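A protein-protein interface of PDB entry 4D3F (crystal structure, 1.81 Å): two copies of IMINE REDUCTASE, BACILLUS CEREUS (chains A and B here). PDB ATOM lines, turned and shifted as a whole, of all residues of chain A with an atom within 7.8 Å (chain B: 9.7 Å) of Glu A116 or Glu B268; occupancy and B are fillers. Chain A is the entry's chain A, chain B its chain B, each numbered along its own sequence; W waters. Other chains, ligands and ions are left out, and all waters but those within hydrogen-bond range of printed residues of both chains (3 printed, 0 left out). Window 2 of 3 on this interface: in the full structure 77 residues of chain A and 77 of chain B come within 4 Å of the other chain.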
ATOM      1  N   TYR A  88       5.957  19.428 -14.707  1.00  0.00           N
ATOM      2  CA  TYR A  88       7.290  18.750 -14.630  1.00  0.00           C
ATOM      3  C   TYR A  88       8.444  19.764 -14.635  1.00  0.00           C
ATOM      4  O   TYR A  88       9.540  19.476 -14.043  1.00  0.00           O
ATOM      5  CB  TYR A  88       7.484  17.757 -15.764  1.00  0.00           C
ATOM      6  CG  TYR A  88       6.889  16.449 -15.509  1.00  0.00           C
ATOM      7  CD1 TYR A  88       5.522  16.196 -15.785  1.00  0.00           C
ATOM      8  CD2 TYR A  88       7.655  15.432 -14.948  1.00  0.00           C
ATOM      9  CE1 TYR A  88       4.972  14.955 -15.512  1.00  0.00           C
ATOM     10  CE2 TYR A  88       7.109  14.191 -14.696  1.00  0.00           C
ATOM     11  CZ  TYR A  88       5.815  13.954 -15.014  1.00  0.00           C
ATOM     12  OH  TYR A  88       5.377  12.728 -14.652  1.00  0.00           O
ATOM     13  N   TYR A  92      12.283  19.803 -12.268  1.00  0.00           N
ATOM     14  CA  TYR A  92      13.663  20.075 -12.619  1.00  0.00           C
ATOM     15  C   TYR A  92      14.224  21.282 -11.912  1.00  0.00           C
ATOM     16  O   TYR A  92      15.411  21.318 -11.481  1.00  0.00           O
ATOM     17  CB  TYR A  92      13.858  20.265 -14.073  1.00  0.00           C
ATOM     18  CG  TYR A  92      13.510  19.063 -14.904  1.00  0.00           C
ATOM     19  CD1 TYR A  92      14.314  17.939 -14.894  1.00  0.00           C
ATOM     20  CD2 TYR A  92      12.352  19.053 -15.703  1.00  0.00           C
ATOM     21  CE1 TYR A  92      14.009  16.811 -15.681  1.00  0.00           C
ATOM     22  CE2 TYR A  92      12.018  17.922 -16.478  1.00  0.00           C
ATOM     23  CZ  TYR A  92      12.868  16.812 -16.466  1.00  0.00           C
ATOM     24  OH  TYR A  92      12.599  15.704 -17.223  1.00  0.00           O
ATOM     25  N   ASP A 113       0.628  15.954 -17.605  1.00  0.00           N
ATOM     26  CA  ASP A 113       1.462  16.253 -18.679  1.00  0.00           C
ATOM     27  C   ASP A 113       1.404  15.078 -19.607  1.00  0.00           C
ATOM     28  O   ASP A 113       0.478  14.246 -19.516  1.00  0.00           O
ATOM     29  CB  ASP A 113       2.918  16.533 -18.168  1.00  0.00           C
ATOM     30  CG  ASP A 113       3.621  17.716 -18.911  1.00  0.00           C
ATOM     31  OD1 ASP A 113       3.549  17.814 -20.175  1.00  0.00           O
ATOM     32  OD2 ASP A 113       4.253  18.536 -18.182  1.00  0.00           O
ATOM     33  N   THR A 114       2.252  15.146 -20.608  1.00  0.00           N
ATOM     34  CA  THR A 114       2.263  14.285 -21.719  1.00  0.00           C
ATOM     35  C   THR A 114       3.085  13.028 -21.366  1.00  0.00           C
ATOM     36  O   THR A 114       3.908  13.056 -20.404  1.00  0.00           O
ATOM     37  CB  THR A 114       2.901  14.921 -22.932  1.00  0.00           C
ATOM     38  OG1 THR A 114       4.324  15.057 -22.789  1.00  0.00           O
ATOM     39  CG2 THR A 114       2.284  16.287 -23.297  1.00  0.00           C
ATOM     40  N   PRO A 115       2.881  11.926 -22.111  1.00  0.00           N
ATOM     41  CA  PRO A 115       3.683  10.742 -21.912  1.00  0.00           C
ATOM     42  C   PRO A 115       5.176  11.037 -22.047  1.00  0.00           C
ATOM     43  O   PRO A 115       5.965  10.496 -21.236  1.00  0.00           O
ATOM     44  CB  PRO A 115       3.180   9.773 -23.011  1.00  0.00           C
ATOM     45  CG  PRO A 115       1.693  10.192 -23.121  1.00  0.00           C
ATOM     46  CD  PRO A 115       1.785  11.693 -23.063  1.00  0.00           C
ATOM     47  N   GLU A 116       5.574  11.759 -23.075  1.00  0.00           N
ATOM     48  CA  GLU A 116       7.041  11.979 -23.262  1.00  0.00           C
ATOM     49  C   GLU A 116       7.643  12.789 -22.088  1.00  0.00           C
ATOM     50  O   GLU A 116       8.806  12.560 -21.685  1.00  0.00           O
ATOM     51  CB  GLU A 116       7.326  12.624 -24.600  1.00  0.00           C
ATOM     52  CG  GLU A 116       8.681  13.299 -24.764  1.00  0.00           C
ATOM     53  CD  GLU A 116       8.808  14.041 -26.137  1.00  0.00           C
ATOM     54  OE1 GLU A 116       7.928  13.918 -27.056  1.00  0.00           O
ATOM     55  OE2 GLU A 116       9.826  14.734 -26.337  1.00  0.00           O
ATOM     56  N   LYS A 117       6.873  13.714 -21.511  1.00  0.00           N
ATOM     57  CA  LYS A 117       7.407  14.499 -20.381  1.00  0.00           C
ATOM     58  C   LYS A 117       7.691  13.545 -19.247  1.00  0.00           C
ATOM     59  O   LYS A 117       8.701  13.677 -18.512  1.00  0.00           O
ATOM     60  CB  LYS A 117       6.447  15.628 -19.934  1.00  0.00           C
ATOM     61  CG  LYS A 117       6.989  17.060 -20.001  1.00  0.00           C
ATOM     62  CD  LYS A 117       6.417  17.857 -21.153  1.00  0.00           C
ATOM     63  N   ALA A 118       6.758  12.627 -18.990  1.00  0.00           N
ATOM     64  CA  ALA A 118       6.942  11.732 -17.896  1.00  0.00           C
ATOM     65  C   ALA A 118       8.127  10.788 -18.170  1.00  0.00           C
ATOM     66  O   ALA A 118       8.862  10.395 -17.222  1.00  0.00           O
ATOM     67  CB  ALA A 118       5.674  10.925 -17.638  1.00  0.00           C
ATOM     68  N   ARG A 119       8.304  10.358 -19.421  1.00  0.00           N
ATOM     69  CA  ARG A 119       9.421   9.482 -19.773  1.00  0.00           C
ATOM     70  C   ARG A 119      10.764  10.200 -19.585  1.00  0.00           C
ATOM     71  O   ARG A 119      11.716   9.584 -19.068  1.00  0.00           O
ATOM     72  CB  ARG A 119       9.355   9.027 -21.215  1.00  0.00           C
ATOM     73  CG  ARG A 119       8.244   7.971 -21.456  1.00  0.00           C
ATOM     74  CD  ARG A 119       7.963   7.806 -22.941  1.00  0.00           C
ATOM     75  NE  ARG A 119       6.758   6.984 -23.052  1.00  0.00           N
ATOM     76  CZ  ARG A 119       5.831   7.133 -24.011  1.00  0.00           C
ATOM     77  NH1 ARG A 119       5.933   8.072 -24.942  1.00  0.00           N
ATOM     78  NH2 ARG A 119       4.765   6.410 -23.967  1.00  0.00           N
ATOM     79  N   LYS A 120      10.836  11.448 -20.031  1.00  0.00           N
ATOM     80  CA  LYS A 120      12.076  12.223 -19.936  1.00  0.00           C
ATOM     81  C   LYS A 120      12.409  12.375 -18.434  1.00  0.00           C
ATOM     82  O   LYS A 120      13.591  12.248 -18.019  1.00  0.00           O
ATOM     83  CB  LYS A 120      11.994  13.566 -20.636  1.00  0.00           C
ATOM     84  CG  LYS A 120      12.141  13.482 -22.184  1.00  0.00           C
ATOM     85  CD  LYS A 120      12.051  14.794 -22.954  1.00  0.00           C
ATOM     86  N   ALA A 121      11.424  12.636 -17.612  1.00  0.00           N
ATOM     87  CA  ALA A 121      11.662  12.775 -16.161  1.00  0.00           C
ATOM     88  C   ALA A 121      12.141  11.528 -15.474  1.00  0.00           C
ATOM     89  O   ALA A 121      13.063  11.573 -14.607  1.00  0.00           O
ATOM     90  CB  ALA A 121      10.422  13.338 -15.446  1.00  0.00           C
ATOM     91  N   ALA A 122      11.553  10.378 -15.816  1.00  0.00           N
ATOM     92  CA  ALA A 122      12.002   9.111 -15.281  1.00  0.00           C
ATOM     93  C   ALA A 122      13.465   8.830 -15.572  1.00  0.00           C
ATOM     94  O   ALA A 122      14.205   8.327 -14.704  1.00  0.00           O
ATOM     95  CB  ALA A 122      11.121   7.961 -15.795  1.00  0.00           C
ATOM     96  N   ASP A 179       6.294   1.333 -18.782  1.00  0.00           N
ATOM     97  CA  ASP A 179       6.582   2.617 -19.389  1.00  0.00           C
ATOM     98  C   ASP A 179       6.047   3.718 -18.529  1.00  0.00           C
ATOM     99  O   ASP A 179       4.826   3.852 -18.298  1.00  0.00           O
ATOM    100  CB  ASP A 179       5.967   2.630 -20.792  1.00  0.00           C
ATOM    101  CG  ASP A 179       5.945   3.973 -21.456  1.00  0.00           C
ATOM    102  OD1 ASP A 179       6.761   4.856 -21.239  1.00  0.00           O
ATOM    103  OD2 ASP A 179       5.044   4.152 -22.306  1.00  0.00           O
ATOM    104  N   PRO A 180       6.947   4.594 -18.094  1.00  0.00           N
ATOM    105  CA  PRO A 180       6.524   5.742 -17.238  1.00  0.00           C
ATOM    106  C   PRO A 180       5.472   6.663 -17.948  1.00  0.00           C
ATOM    107  O   PRO A 180       4.746   7.316 -17.297  1.00  0.00           O
ATOM    108  CB  PRO A 180       7.844   6.526 -17.022  1.00  0.00           C
ATOM    109  CG  PRO A 180       8.945   5.496 -17.279  1.00  0.00           C
ATOM    110  CD  PRO A 180       8.406   4.613 -18.393  1.00  0.00           C
ATOM    111  N   GLY A 181       5.459   6.688 -19.269  1.00  0.00           N
ATOM    112  CA  GLY A 181       4.509   7.472 -20.004  1.00  0.00           C
ATOM    113  C   GLY A 181       3.072   6.965 -19.957  1.00  0.00           C
ATOM    114  O   GLY A 181       2.128   7.706 -20.241  1.00  0.00           O
ATOM    115  N   LEU A 182       2.857   5.719 -19.551  1.00  0.00           N
ATOM    116  CA  LEU A 182       1.497   5.122 -19.710  1.00  0.00           C
ATOM    117  C   LEU A 182       0.437   5.706 -18.813  1.00  0.00           C
ATOM    118  O   LEU A 182      -0.742   5.825 -19.226  1.00  0.00           O
ATOM    119  CB  LEU A 182       1.607   3.628 -19.451  1.00  0.00           C
ATOM    120  CG  LEU A 182       1.780   2.612 -20.538  1.00  0.00           C
ATOM    121  CD1 LEU A 182       1.789   3.007 -21.988  1.00  0.00           C
ATOM    122  CD2 LEU A 182       2.602   1.395 -20.145  1.00  0.00           C
ATOM    123  N   MET A 184       0.079   8.752 -17.977  1.00  0.00           N
ATOM    124  CA  MET A 184      -0.336   9.974 -18.601  1.00  0.00           C
ATOM    125  C   MET A 184      -1.043   9.596 -19.934  1.00  0.00           C
ATOM    126  O   MET A 184      -1.985  10.270 -20.332  1.00  0.00           O
ATOM    127  CB  MET A 184       0.866  10.859 -18.898  1.00  0.00           C
ATOM    128  CG  MET A 184       1.564  11.434 -17.605  1.00  0.00           C
ATOM    129  SD  MET A 184       0.575  11.852 -16.154  1.00  0.00           S
ATOM    130  CE  MET A 184      -0.383  12.793 -17.171  1.00  0.00           C
ATOM    131  N   LEU A 185      -0.572   8.572 -20.619  1.00  0.00           N
ATOM    132  CA  LEU A 185      -1.243   8.142 -21.907  1.00  0.00           C
ATOM    133  C   LEU A 185      -2.748   7.870 -21.693  1.00  0.00           C
ATOM    134  O   LEU A 185      -3.609   8.498 -22.365  1.00  0.00           O
ATOM    135  CB  LEU A 185      -0.548   6.976 -22.527  1.00  0.00           C
ATOM    136  CG  LEU A 185      -1.197   6.453 -23.850  1.00  0.00           C
ATOM    137  CD1 LEU A 185      -0.974   7.469 -24.970  1.00  0.00           C
ATOM    138  CD2 LEU A 185      -0.659   5.113 -24.123  1.00  0.00           C
ATOM    139  N   HIS B 203      -9.287   9.009 -33.051  1.00  0.00           N
ATOM    140  CA  HIS B 203      -8.132   9.935 -32.813  1.00  0.00           C
ATOM    141  C   HIS B 203      -7.349   9.516 -31.561  1.00  0.00           C
ATOM    142  O   HIS B 203      -6.122   9.346 -31.599  1.00  0.00           O
ATOM    143  CB  HIS B 203      -8.665  11.348 -32.686  1.00  0.00           C
ATOM    144  CG  HIS B 203      -7.565  12.350 -32.582  1.00  0.00           C
ATOM    145  ND1 HIS B 203      -7.056  12.724 -31.379  1.00  0.00           N
ATOM    146  CD2 HIS B 203      -6.824  12.970 -33.532  1.00  0.00           C
ATOM    147  CE1 HIS B 203      -6.046  13.562 -31.581  1.00  0.00           C
ATOM    148  NE2 HIS B 203      -5.890  13.721 -32.886  1.00  0.00           N
ATOM    149  N   ALA B 206      -5.497   6.305 -32.236  1.00  0.00           N
ATOM    150  CA  ALA B 206      -4.266   6.531 -32.977  1.00  0.00           C
ATOM    151  C   ALA B 206      -3.115   6.956 -32.047  1.00  0.00           C
ATOM    152  O   ALA B 206      -1.956   6.524 -32.235  1.00  0.00           O
ATOM    153  CB  ALA B 206      -4.460   7.546 -34.063  1.00  0.00           C
ATOM    154  N   ILE B 207      -3.406   7.837 -31.110  1.00  0.00           N
ATOM    155  CA  ILE B 207      -2.373   8.215 -30.117  1.00  0.00           C
ATOM    156  C   ILE B 207      -1.952   6.975 -29.331  1.00  0.00           C
ATOM    157  O   ILE B 207      -0.766   6.750 -29.082  1.00  0.00           O
ATOM    158  CB  ILE B 207      -2.929   9.284 -29.152  1.00  0.00           C
ATOM    159  CG1 ILE B 207      -3.314  10.556 -29.903  1.00  0.00           C
ATOM    160  CG2 ILE B 207      -1.922   9.562 -28.021  1.00  0.00           C
ATOM    161  CD1 ILE B 207      -4.013  11.611 -29.029  1.00  0.00           C
ATOM    162  N   ALA B 210       0.297   4.758 -31.414  1.00  0.00           N
ATOM    163  CA  ALA B 210       1.610   5.329 -31.553  1.00  0.00           C
ATOM    164  C   ALA B 210       2.480   5.065 -30.315  1.00  0.00           C
ATOM    165  O   ALA B 210       3.698   4.928 -30.457  1.00  0.00           O
ATOM    166  CB  ALA B 210       1.560   6.823 -31.816  1.00  0.00           C
ATOM    167  N   ASN B 211       1.860   5.004 -29.169  1.00  0.00           N
ATOM    168  CA  ASN B 211       2.510   4.760 -27.915  1.00  0.00           C
ATOM    169  C   ASN B 211       2.607   3.297 -27.518  1.00  0.00           C
ATOM    170  O   ASN B 211       3.158   3.011 -26.457  1.00  0.00           O
ATOM    171  CB  ASN B 211       1.820   5.539 -26.796  1.00  0.00           C
ATOM    172  CG  ASN B 211       2.216   7.003 -26.771  1.00  0.00           C
ATOM    173  OD1 ASN B 211       3.202   7.403 -26.083  1.00  0.00           O
ATOM    174  ND2 ASN B 211       1.520   7.809 -27.583  1.00  0.00           N
ATOM    175  N   GLU B 260      -5.138  21.727 -23.899  1.00  0.00           N
ATOM    176  CA  GLU B 260      -3.784  21.912 -24.321  1.00  0.00           C
ATOM    177  C   GLU B 260      -2.879  20.684 -24.126  1.00  0.00           C
ATOM    178  O   GLU B 260      -2.077  20.428 -25.016  1.00  0.00           O
ATOM    179  CB  GLU B 260      -3.149  23.118 -23.521  1.00  0.00           C
ATOM    180  CG  GLU B 260      -3.656  24.467 -24.025  1.00  0.00           C
ATOM    181  CD  GLU B 260      -3.195  25.636 -23.128  1.00  0.00           C
ATOM    182  OE1 GLU B 260      -2.755  25.374 -22.024  1.00  0.00           O
ATOM    183  OE2 GLU B 260      -3.351  26.803 -23.527  1.00  0.00           O
ATOM    184  N   HIS B 261      -3.054  19.967 -23.028  1.00  0.00           N
ATOM    185  CA  HIS B 261      -2.248  18.748 -22.762  1.00  0.00           C
ATOM    186  C   HIS B 261      -2.630  17.646 -23.790  1.00  0.00           C
ATOM    187  O   HIS B 261      -1.759  16.912 -24.284  1.00  0.00           O
ATOM    188  CB  HIS B 261      -2.436  18.212 -21.416  1.00  0.00           C
ATOM    189  CG  HIS B 261      -1.826  19.058 -20.317  1.00  0.00           C
ATOM    190  ND1 HIS B 261      -0.572  19.610 -20.405  1.00  0.00           N
ATOM    191  CD2 HIS B 261      -2.294  19.378 -19.090  1.00  0.00           C
ATOM    192  CE1 HIS B 261      -0.298  20.276 -19.283  1.00  0.00           C
ATOM    193  NE2 HIS B 261      -1.336  20.161 -18.475  1.00  0.00           N
ATOM    194  N   VAL B 262      -3.913  17.619 -24.177  1.00  0.00           N
ATOM    195  CA  VAL B 262      -4.366  16.706 -25.217  1.00  0.00           C
ATOM    196  C   VAL B 262      -3.706  17.029 -26.546  1.00  0.00           C
ATOM    197  O   VAL B 262      -3.185  16.141 -27.229  1.00  0.00           O
ATOM    198  CB  VAL B 262      -5.920  16.690 -25.355  1.00  0.00           C
ATOM    199  CG1 VAL B 262      -6.271  15.919 -26.607  1.00  0.00           C
ATOM    200  CG2 VAL B 262      -6.508  16.083 -24.128  1.00  0.00           C
ATOM    201  N   VAL B 263      -3.696  18.306 -26.962  1.00  0.00           N
ATOM    202  CA  VAL B 263      -3.034  18.722 -28.172  1.00  0.00           C
ATOM    203  C   VAL B 263      -1.537  18.357 -28.132  1.00  0.00           C
ATOM    204  O   VAL B 263      -0.958  17.915 -29.155  1.00  0.00           O
ATOM    205  CB  VAL B 263      -3.269  20.224 -28.441  1.00  0.00           C
ATOM    206  CG1 VAL B 263      -2.381  20.766 -29.528  1.00  0.00           C
ATOM    207  CG2 VAL B 263      -4.762  20.439 -28.774  1.00  0.00           C
ATOM    208  N   HIS B 264      -0.867  18.640 -27.026  1.00  0.00           N
ATOM    209  CA  HIS B 264       0.599  18.358 -26.968  1.00  0.00           C
ATOM    210  C   HIS B 264       0.849  16.847 -27.027  1.00  0.00           C
ATOM    211  O   HIS B 264       1.754  16.413 -27.681  1.00  0.00           O
ATOM    212  CB  HIS B 264       1.203  18.878 -25.669  1.00  0.00           C
ATOM    213  CG  HIS B 264       1.217  20.343 -25.583  1.00  0.00           C
ATOM    214  ND1 HIS B 264       1.217  21.018 -24.374  1.00  0.00           N
ATOM    215  CD2 HIS B 264       1.170  21.290 -26.550  1.00  0.00           C
ATOM    216  CE1 HIS B 264       1.235  22.319 -24.611  1.00  0.00           C
ATOM    217  NE2 HIS B 264       1.151  22.509 -25.913  1.00  0.00           N
ATOM    218  N   THR B 265      -0.008  16.032 -26.405  1.00  0.00           N
ATOM    219  CA  THR B 265       0.123  14.592 -26.451  1.00  0.00           C
ATOM    220  C   THR B 265      -0.018  14.096 -27.874  1.00  0.00           C
ATOM    221  O   THR B 265       0.713  13.237 -28.352  1.00  0.00           O
ATOM    222  CB  THR B 265      -0.949  13.971 -25.560  1.00  0.00           C
ATOM    223  OG1 THR B 265      -0.713  14.355 -24.218  1.00  0.00           O
ATOM    224  CG2 THR B 265      -1.013  12.400 -25.627  1.00  0.00           C
ATOM    225  N   THR B 266      -0.996  14.669 -28.578  1.00  0.00           N
ATOM    226  CA  THR B 266      -1.205  14.374 -29.998  1.00  0.00           C
ATOM    227  C   THR B 266       0.034  14.652 -30.848  1.00  0.00           C
ATOM    228  O   THR B 266       0.486  13.854 -31.695  1.00  0.00           O
ATOM    229  CB  THR B 266      -2.418  15.207 -30.551  1.00  0.00           C
ATOM    230  OG1 THR B 266      -3.580  14.917 -29.768  1.00  0.00           O
ATOM    231  CG2 THR B 266      -2.684  14.888 -31.959  1.00  0.00           C
ATOM    232  N   GLN B 267       0.564  15.845 -30.660  1.00  0.00           N
ATOM    233  CA  GLN B 267       1.735  16.244 -31.430  1.00  0.00           C
ATOM    234  C   GLN B 267       2.925  15.382 -31.147  1.00  0.00           C
ATOM    235  O   GLN B 267       3.640  15.051 -32.053  1.00  0.00           O
ATOM    236  CB  GLN B 267       2.154  17.712 -31.101  1.00  0.00           C
ATOM    237  CG  GLN B 267       1.194  18.749 -31.577  1.00  0.00           C
ATOM    238  CD  GLN B 267       1.448  20.157 -30.980  1.00  0.00           C
ATOM    239  OE1 GLN B 267       1.820  20.363 -29.800  1.00  0.00           O
ATOM    240  NE2 GLN B 267       1.173  21.112 -31.785  1.00  0.00           N
ATOM    241  N   GLU B 268       3.160  15.070 -29.911  1.00  0.00           N
ATOM    242  CA  GLU B 268       4.290  14.189 -29.523  1.00  0.00           C
ATOM    243  C   GLU B 268       4.188  12.783 -30.155  1.00  0.00           C
ATOM    244  O   GLU B 268       5.170  12.103 -30.369  1.00  0.00           O
ATOM    245  CB  GLU B 268       4.263  13.988 -28.020  1.00  0.00           C
ATOM    246  CG  GLU B 268       4.778  15.174 -27.235  1.00  0.00           C
ATOM    247  CD  GLU B 268       4.698  15.000 -25.717  1.00  0.00           C
ATOM    248  OE1 GLU B 268       4.329  13.876 -25.208  1.00  0.00           O
ATOM    249  OE2 GLU B 268       4.963  16.022 -25.056  1.00  0.00           O
ATOM    250  N   ALA B 269       2.967  12.335 -30.396  1.00  0.00           N
ATOM    251  CA  ALA B 269       2.745  11.026 -30.951  1.00  0.00           C
ATOM    252  C   ALA B 269       2.753  11.080 -32.455  1.00  0.00           C
ATOM    253  O   ALA B 269       2.511  10.070 -33.077  1.00  0.00           O
ATOM    254  CB  ALA B 269       1.386  10.506 -30.442  1.00  0.00           C
ATOM    255  N   GLY B 270       2.921  12.250 -33.040  1.00  0.00           N
ATOM    256  CA  GLY B 270       2.894  12.435 -34.452  1.00  0.00           C
ATOM    257  C   GLY B 270       1.539  12.278 -35.116  1.00  0.00           C
ATOM    258  O   GLY B 270       1.459  11.994 -36.307  1.00  0.00           O
ATOM    259  N   ILE B 271       0.486  12.481 -34.348  1.00  0.00           N
ATOM    260  CA  ILE B 271      -0.904  12.237 -34.794  1.00  0.00           C
ATOM    261  C   ILE B 271      -1.503  13.528 -35.302  1.00  0.00           C
ATOM    262  O   ILE B 271      -1.148  14.623 -34.854  1.00  0.00           O
ATOM    263  CB  ILE B 271      -1.717  11.630 -33.667  1.00  0.00           C
ATOM    264  CG1 ILE B 271      -1.159  10.222 -33.270  1.00  0.00           C
ATOM    265  CG2 ILE B 271      -3.191  11.544 -34.012  1.00  0.00           C
ATOM    266  CD1 ILE B 271      -0.978   9.234 -34.428  1.00  0.00           C
ATOM    267  N   ASP B 272      -2.341  13.427 -36.315  1.00  0.00           N
ATOM    268  CA  ASP B 272      -2.984  14.583 -36.934  1.00  0.00           C
ATOM    269  C   ASP B 272      -3.682  15.473 -35.898  1.00  0.00           C
ATOM    270  O   ASP B 272      -4.464  14.988 -35.082  1.00  0.00           O
ATOM    271  CB  ASP B 272      -4.034  14.117 -37.937  1.00  0.00           C
ATOM    272  CG  ASP B 272      -4.558  15.278 -38.819  1.00  0.00           C
ATOM    273  OD1 ASP B 272      -3.823  15.801 -39.644  1.00  0.00           O
ATOM    274  OD2 ASP B 272      -5.734  15.629 -38.711  1.00  0.00           O
ATOM    275  N   ILE B 273      -3.419  16.755 -35.927  1.00  0.00           N
ATOM    276  CA  ILE B 273      -3.928  17.626 -34.825  1.00  0.00           C
ATOM    277  C   ILE B 273      -5.280  18.259 -35.172  1.00  0.00           C
ATOM    278  O   ILE B 273      -5.792  18.948 -34.347  1.00  0.00           O
ATOM    279  CB  ILE B 273      -3.042  18.827 -34.365  1.00  0.00           C
ATOM    280  CG1 ILE B 273      -2.334  19.437 -35.515  1.00  0.00           C
ATOM    281  CG2 ILE B 273      -2.267  18.537 -33.085  1.00  0.00           C
ATOM    282  CD1 ILE B 273      -3.234  20.204 -36.424  1.00  0.00           C
HETATM  283  O   HOH W   1       1.477  19.704 -22.163  1.00  0.00           O
HETATM  284  O   HOH W   2       4.595   9.803 -27.310  1.00  0.00           O
HETATM  285  O   HOH W   3       7.593  12.445 -29.682  1.00  0.00           O
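The side-chain carboxylate (OE2) of Glu B268 lies within hydrogen-bond range of the side-chain hydroxyl (OG1) of Thr A114, at 2.5 Å.
The guanidinium group (NH2) of Arg A119 lies within hydrogen-bond range of the side-chain amide oxygen (OD1) of Asn B211 (2.8 Å).
The backbone NH of Glu A116 sits at hydrogen-bond distance from the side-chain carboxylate of Glu B268 (3.3 Å).
O of His B261 lies within hydrogen-bond range of OG1 of Thr B265 (2.8 Å).
O of Ile B207 lies within hydrogen-bond range of ND2 of Asn B211, at 2.9 Å.
The guanidinium group (NE) of Arg A119 is in salt-bridge range of the side-chain carboxylate (OD1) of Asp A179, at 2.8 Å.
The side-chain hydroxyl of Thr A114 is in hydrogen-bond range of the backbone NH of Lys A117 (3.2 Å).
A ring nitrogen (ND1) of His B264 lies close to the backbone carbonyl oxygen (O) of Glu B260 (3.4 Å).
Thr A114 touches His B264.
OG1 of Thr B265 touches CG2 of Thr A114, 3.7 Å away.
Asn B211 touches Pro A115 (OD1 to CB, 3.9 Å).
Thr B265 touches Pro A115 (OG1 to CD, 3.8 Å).
OE1 of Glu B268 touches N of Pro A115, at 3.9 Å.
Ile B207 touches Leu A185.
Asn B211 touches Leu A185 (ND2 to CD1, 3.6 Å).
Glu A116 touches just one residue of chain B: Glu B268.
Thr A114 touches just these residues of chain B: His B264, Thr B265 and Glu B268.
Pro A115 touches just these residues of chain B: Asn B211 (3.9 Å), Thr B265 (3.8 Å) and Glu B268 (3.9 Å).
No residue of chain B comes within 4 Å of Ala A118.
Printed residues of chain B within 4 Å of Leu A185: Ile B207 (3.8 Å) and Asn B211 (3.6 Å).
Of the printed residues of chain A, Asn B211 touches Pro A115 (3.9 Å), Arg A119 (2.8 Å) and Leu A185 (3.6 Å).
Thr B266 touches none of the printed residues of chain A.
Gly A181 touches none of the printed residues of chain B.
The nearest printed residue of chain A that does not touch Thr B265 is Asp A113 (4.9 Å).
Among the printed residues, 10 pairs touch across the chains.
No position is printed for both chains.
Of the 10 pairs that touch across the chains among the printed residues, none has its exchanged pair printed and touching as well.
Water W3 bridges the backbone carbonyl oxygen of Glu B268 and the side-chain carboxylate of Glu A116.
Water W1 lies within hydrogen-bond range of a ring nitrogen (ND1) of His B264 (2.6 Å), a ring nitrogen (ND1) of His B261 (2.7 Å) and the side-chain carboxylate of Asp A113 (3.4 Å).
Water W2 bridges OD1 of Asn B211 and NH1 of Arg A119.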
